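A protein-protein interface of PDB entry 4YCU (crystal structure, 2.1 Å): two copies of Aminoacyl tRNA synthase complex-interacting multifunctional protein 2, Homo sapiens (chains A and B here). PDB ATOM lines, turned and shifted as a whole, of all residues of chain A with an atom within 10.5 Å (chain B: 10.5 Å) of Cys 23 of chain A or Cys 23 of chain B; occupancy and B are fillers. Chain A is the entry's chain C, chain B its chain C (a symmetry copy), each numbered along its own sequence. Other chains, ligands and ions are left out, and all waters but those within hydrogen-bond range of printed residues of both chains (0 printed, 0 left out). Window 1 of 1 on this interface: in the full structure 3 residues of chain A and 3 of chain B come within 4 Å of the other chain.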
ATOM      1  N   LEU A  20      -0.091 -11.161 -20.604  1.00  0.00           N
ATOM      2  CA  LEU A  20       0.780 -11.315 -21.764  1.00  0.00           C
ATOM      3  C   LEU A  20       0.862 -12.775 -22.210  1.00  0.00           C
ATOM      4  O   LEU A  20       0.540 -13.676 -21.436  1.00  0.00           O
ATOM      5  CB  LEU A  20       2.174 -10.778 -21.433  1.00  0.00           C
ATOM      6  CG  LEU A  20       2.267  -9.264 -21.245  1.00  0.00           C
ATOM      7  CD1 LEU A  20       3.660  -8.871 -20.787  1.00  0.00           C
ATOM      8  CD2 LEU A  20       1.891  -8.539 -22.528  1.00  0.00           C
ATOM      9  N   PRO A  21       1.287 -13.014 -23.466  1.00  0.00           N
ATOM     10  CA  PRO A  21       1.465 -14.387 -23.958  1.00  0.00           C
ATOM     11  C   PRO A  21       2.471 -15.170 -23.121  1.00  0.00           C
ATOM     12  O   PRO A  21       3.339 -14.564 -22.493  1.00  0.00           O
ATOM     13  CB  PRO A  21       1.979 -14.181 -25.386  1.00  0.00           C
ATOM     14  CG  PRO A  21       1.450 -12.842 -25.774  1.00  0.00           C
ATOM     15  CD  PRO A  21       1.551 -12.025 -24.526  1.00  0.00           C
ATOM     16  N   THR A  22       2.375 -16.499 -23.129  1.00  0.00           N
ATOM     17  CA  THR A  22       3.194 -17.298 -22.220  1.00  0.00           C
ATOM     18  C   THR A  22       3.714 -18.578 -22.846  1.00  0.00           C
ATOM     19  O   THR A  22       3.240 -19.002 -23.909  1.00  0.00           O
ATOM     20  CB  THR A  22       2.391 -17.710 -20.961  1.00  0.00           C
ATOM     21  OG1 THR A  22       1.217 -18.436 -21.354  1.00  0.00           O
ATOM     22  CG2 THR A  22       1.984 -16.493 -20.140  1.00  0.00           C
ATOM     23  N   CYS A  23       4.725 -19.171 -22.190  1.00  0.00           N
ATOM     24  CA  CYS A  23       5.383 -20.275 -22.853  1.00  0.00           C
ATOM     25  C   CYS A  23       5.708 -21.299 -21.726  1.00  0.00           C
ATOM     26  O   CYS A  23       6.345 -20.949 -20.721  1.00  0.00           O
ATOM     27  CB  CYS A  23       6.603 -19.767 -23.625  1.00  0.00           C
ATOM     28  SG  CYS A  23       7.590 -21.024 -24.462  1.00  0.00           S
ATOM     29  N   MET A  24       5.227 -22.529 -21.866  1.00  0.00           N
ATOM     30  CA  MET A  24       5.459 -23.581 -20.877  1.00  0.00           C
ATOM     31  C   MET A  24       6.956 -23.792 -20.654  1.00  0.00           C
ATOM     32  O   MET A  24       7.699 -24.012 -21.608  1.00  0.00           O
ATOM     33  CB  MET A  24       4.811 -24.888 -21.338  1.00  0.00           C
ATOM     34  CG  MET A  24       5.072 -26.067 -20.431  1.00  0.00           C
ATOM     35  SD  MET A  24       3.719 -26.223 -19.255  1.00  0.00           S
ATOM     36  CE  MET A  24       4.509 -27.153 -17.944  1.00  0.00           C
ATOM     37  N   TYR A  25       7.402 -23.709 -19.401  1.00  0.00           N
ATOM     38  CA  TYR A  25       8.830 -23.820 -19.108  1.00  0.00           C
ATOM     39  C   TYR A  25       9.326 -25.227 -19.406  1.00  0.00           C
ATOM     40  O   TYR A  25       8.535 -26.164 -19.511  1.00  0.00           O
ATOM     41  CB  TYR A  25       9.124 -23.459 -17.649  1.00  0.00           C
ATOM     42  CG  TYR A  25       8.848 -24.575 -16.658  1.00  0.00           C
ATOM     43  CD1 TYR A  25       9.848 -25.037 -15.811  1.00  0.00           C
ATOM     44  CD2 TYR A  25       7.590 -25.155 -16.563  1.00  0.00           C
ATOM     45  CE1 TYR A  25       9.604 -26.052 -14.901  1.00  0.00           C
ATOM     46  CE2 TYR A  25       7.337 -26.170 -15.656  1.00  0.00           C
ATOM     47  CZ  TYR A  25       8.347 -26.613 -14.828  1.00  0.00           C
ATOM     48  OH  TYR A  25       8.099 -27.622 -13.927  1.00  0.00           O
ATOM     49  N   ARG A  26      10.638 -25.379 -19.534  1.00  0.00           N
ATOM     50  CA  ARG A  26      11.207 -26.688 -19.823  1.00  0.00           C
ATOM     51  C   ARG A  26      12.197 -27.171 -18.765  1.00  0.00           C
ATOM     52  O   ARG A  26      12.896 -26.373 -18.140  1.00  0.00           O
ATOM     53  CB  ARG A  26      11.870 -26.643 -21.198  1.00  0.00           C
ATOM     54  CG  ARG A  26      11.974 -27.977 -21.907  1.00  0.00           C
ATOM     55  CD  ARG A  26      12.673 -27.793 -23.240  1.00  0.00           C
ATOM     56  NE  ARG A  26      11.748 -27.250 -24.232  1.00  0.00           N
ATOM     57  CZ  ARG A  26      12.065 -26.996 -25.497  1.00  0.00           C
ATOM     58  NH1 ARG A  26      13.294 -27.229 -25.937  1.00  0.00           N
ATOM     59  NH2 ARG A  26      11.151 -26.506 -26.324  1.00  0.00           N
ATOM     60  N   LEU A  27      12.243 -28.485 -18.571  1.00  0.00           N
ATOM     61  CA  LEU A  27      13.247 -29.111 -17.720  1.00  0.00           C
ATOM     62  C   LEU A  27      14.304 -29.816 -18.573  1.00  0.00           C
ATOM     63  O   LEU A  27      14.020 -30.219 -19.700  1.00  0.00           O
ATOM     64  CB  LEU A  27      12.577 -30.098 -16.760  1.00  0.00           C
ATOM     65  CG  LEU A  27      11.669 -29.466 -15.704  1.00  0.00           C
ATOM     66  CD1 LEU A  27      10.914 -30.530 -14.924  1.00  0.00           C
ATOM     67  CD2 LEU A  27      12.487 -28.597 -14.766  1.00  0.00           C
ATOM     68  N   LEU B  20      10.762 -30.213 -31.391  1.00  0.00           N
ATOM     69  CA  LEU B  20      10.241 -29.961 -30.052  1.00  0.00           C
ATOM     70  C   LEU B  20       9.331 -28.733 -30.029  1.00  0.00           C
ATOM     71  O   LEU B  20       9.386 -27.906 -30.940  1.00  0.00           O
ATOM     72  CB  LEU B  20      11.405 -29.782 -29.075  1.00  0.00           C
ATOM     73  CG  LEU B  20      12.227 -31.039 -28.795  1.00  0.00           C
ATOM     74  CD1 LEU B  20      13.428 -30.705 -27.927  1.00  0.00           C
ATOM     75  CD2 LEU B  20      11.366 -32.111 -28.144  1.00  0.00           C
ATOM     76  N   PRO B  21       8.482 -28.612 -28.991  1.00  0.00           N
ATOM     77  CA  PRO B  21       7.620 -27.431 -28.849  1.00  0.00           C
ATOM     78  C   PRO B  21       8.426 -26.141 -28.758  1.00  0.00           C
ATOM     79  O   PRO B  21       9.587 -26.179 -28.349  1.00  0.00           O
ATOM     80  CB  PRO B  21       6.869 -27.704 -27.541  1.00  0.00           C
ATOM     81  CG  PRO B  21       6.872 -29.189 -27.422  1.00  0.00           C
ATOM     82  CD  PRO B  21       8.216 -29.602 -27.931  1.00  0.00           C
ATOM     83  N   THR B  22       7.818 -25.009 -29.110  1.00  0.00           N
ATOM     84  CA  THR B  22       8.581 -23.766 -29.211  1.00  0.00           C
ATOM     85  C   THR B  22       7.824 -22.553 -28.706  1.00  0.00           C
ATOM     86  O   THR B  22       6.601 -22.604 -28.510  1.00  0.00           O
ATOM     87  CB  THR B  22       8.974 -23.470 -30.679  1.00  0.00           C
ATOM     88  OG1 THR B  22       7.792 -23.403 -31.491  1.00  0.00           O
ATOM     89  CG2 THR B  22       9.909 -24.539 -31.230  1.00  0.00           C
ATOM     90  N   CYS B  23       8.575 -21.467 -28.461  1.00  0.00           N
ATOM     91  CA  CYS B  23       7.931 -20.358 -27.790  1.00  0.00           C
ATOM     92  C   CYS B  23       8.524 -19.077 -28.449  1.00  0.00           C
ATOM     93  O   CYS B  23       9.751 -18.905 -28.500  1.00  0.00           O
ATOM     94  CB  CYS B  23       8.156 -20.462 -26.280  1.00  0.00           C
ATOM     95  SG  CYS B  23       7.477 -19.118 -25.285  1.00  0.00           S
ATOM     96  N   MET B  24       7.665 -18.223 -28.993  1.00  0.00           N
ATOM     97  CA  MET B  24       8.095 -16.985 -29.644  1.00  0.00           C
ATOM     98  C   MET B  24       8.915 -16.125 -28.682  1.00  0.00           C
ATOM     99  O   MET B  24       8.460 -15.824 -27.580  1.00  0.00           O
ATOM    100  CB  MET B  24       6.877 -16.201 -30.137  1.00  0.00           C
ATOM    101  CG  MET B  24       7.205 -14.856 -30.743  1.00  0.00           C
ATOM    102  SD  MET B  24       7.371 -15.033 -32.526  1.00  0.00           S
ATOM    103  CE  MET B  24       8.372 -13.602 -32.921  1.00  0.00           C
ATOM    104  N   TYR B  25      10.125 -15.744 -29.088  1.00  0.00           N
ATOM    105  CA  TYR B  25      11.006 -14.987 -28.200  1.00  0.00           C
ATOM    106  C   TYR B  25      10.434 -13.600 -27.942  1.00  0.00           C
ATOM    107  O   TYR B  25       9.573 -13.127 -28.681  1.00  0.00           O
ATOM    108  CB  TYR B  25      12.415 -14.870 -28.788  1.00  0.00           C
ATOM    109  CG  TYR B  25      12.569 -13.789 -29.842  1.00  0.00           C
ATOM    110  CD1 TYR B  25      13.515 -12.781 -29.694  1.00  0.00           C
ATOM    111  CD2 TYR B  25      11.779 -13.782 -30.984  1.00  0.00           C
ATOM    112  CE1 TYR B  25      13.665 -11.793 -30.652  1.00  0.00           C
ATOM    113  CE2 TYR B  25      11.922 -12.799 -31.947  1.00  0.00           C
ATOM    114  CZ  TYR B  25      12.866 -11.808 -31.776  1.00  0.00           C
ATOM    115  OH  TYR B  25      13.011 -10.828 -32.730  1.00  0.00           O
ATOM    116  N   ARG B  26      10.919 -12.945 -26.894  1.00  0.00           N
ATOM    117  CA  ARG B  26      10.431 -11.613 -26.564  1.00  0.00           C
ATOM    118  C   ARG B  26      11.525 -10.547 -26.556  1.00  0.00           C
ATOM    119  O   ARG B  26      12.680 -10.825 -26.233  1.00  0.00           O
ATOM    120  CB  ARG B  26       9.727 -11.670 -25.210  1.00  0.00           C
ATOM    121  CG  ARG B  26       8.680 -10.600 -24.984  1.00  0.00           C
ATOM    122  CD  ARG B  26       8.084 -10.755 -23.597  1.00  0.00           C
ATOM    123  NE  ARG B  26       7.098 -11.833 -23.583  1.00  0.00           N
ATOM    124  CZ  ARG B  26       6.394 -12.196 -22.515  1.00  0.00           C
ATOM    125  NH1 ARG B  26       6.567 -11.570 -21.359  1.00  0.00           N
ATOM    126  NH2 ARG B  26       5.518 -13.188 -22.604  1.00  0.00           N
ATOM    127  N   LEU B  27      11.146  -9.326 -26.920  1.00  0.00           N
ATOM    128  CA  LEU B  27      12.028  -8.171 -26.806  1.00  0.00           C
ATOM    129  C   LEU B  27      11.604  -7.290 -25.631  1.00  0.00           C
ATOM    130  O   LEU B  27      10.435  -7.294 -25.247  1.00  0.00           O
ATOM    131  CB  LEU B  27      12.019  -7.375 -28.114  1.00  0.00           C
ATOM    132  CG  LEU B  27      12.642  -8.087 -29.316  1.00  0.00           C
ATOM    133  CD1 LEU B  27      12.420  -7.296 -30.595  1.00  0.00           C
ATOM    134  CD2 LEU B  27      14.124  -8.312 -29.077  1.00  0.00           C
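Pro 21 of chain A touches Arg 26 of chain B, and with the chains exchanged Arg 26 of chain A touches Pro 21 of chain B.
Cys 23 of chain A touches its own counterpart, Cys 23 of chain B.
Of the 3 pairs that touch across the chains among the printed residues, 3 have their exchanged pair printed and touching as well.
Of chain B, only Cys 23 comes within 4 Å of Cys 23 of chain A.
Cys 23 of chain B touches just one residue of chain A: Cys 23 (2.0 Å).
Thr 22 of chain A touches none of the printed residues of chain B.
Of the printed residues of chain B, Arg 26 of chain A touches Pro 21.
Of the printed residues of chain B, Pro 21 of chain A touches Arg 26 (2.6 Å).
Printed residues of chain A within 4 Å of Pro 21 of chain B: Arg 26 (2.6 Å).
Leu 27 of chain A touches none of the printed residues of chain B.
Leu 27 of chain B touches none of the printed residues of chain A.
The nearest residue of chain A that does not touch Cys 23 of chain B is Thr 22 of chain A (4.5 Å).
The nearest printed residue of chain A that does not touch Pro 21 of chain B is Cys 23 of chain A (6.7 Å).
Of the 8 printed residues of chain A, 3 touch a printed residue of chain B.
Printed residues of chain A that touch a printed residue of chain B: Pro 21, Cys 23 and Arg 26.
Of the 8 printed residues of chain B, 3 touch a printed residue of chain A.
Along chain B the printed residues that touch a printed residue of chain A span positions 21 to 26.
Among the printed residues, 3 pairs touch across the chains.
Among the printed residues, no Asp or Glu carboxylate lies within 4 Å of a Lys or Arg side-chain nitrogen of the other chain.
The backbone carbonyl oxygen (O) of Pro 21 of chain A lies within hydrogen-bond range of the guanidinium group (NH2) of Arg 26 of chain B (2.6 Å).
SG of Cys 23 of chain A is disulfide-bonded to SG of Cys 23 of chain B (2.1 Å).
The guanidinium group (NH2) of Arg 26 of chain A sits at hydrogen-bond distance from the backbone carbonyl oxygen (O) of Pro 21 of chain B, at 2.6 Å.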
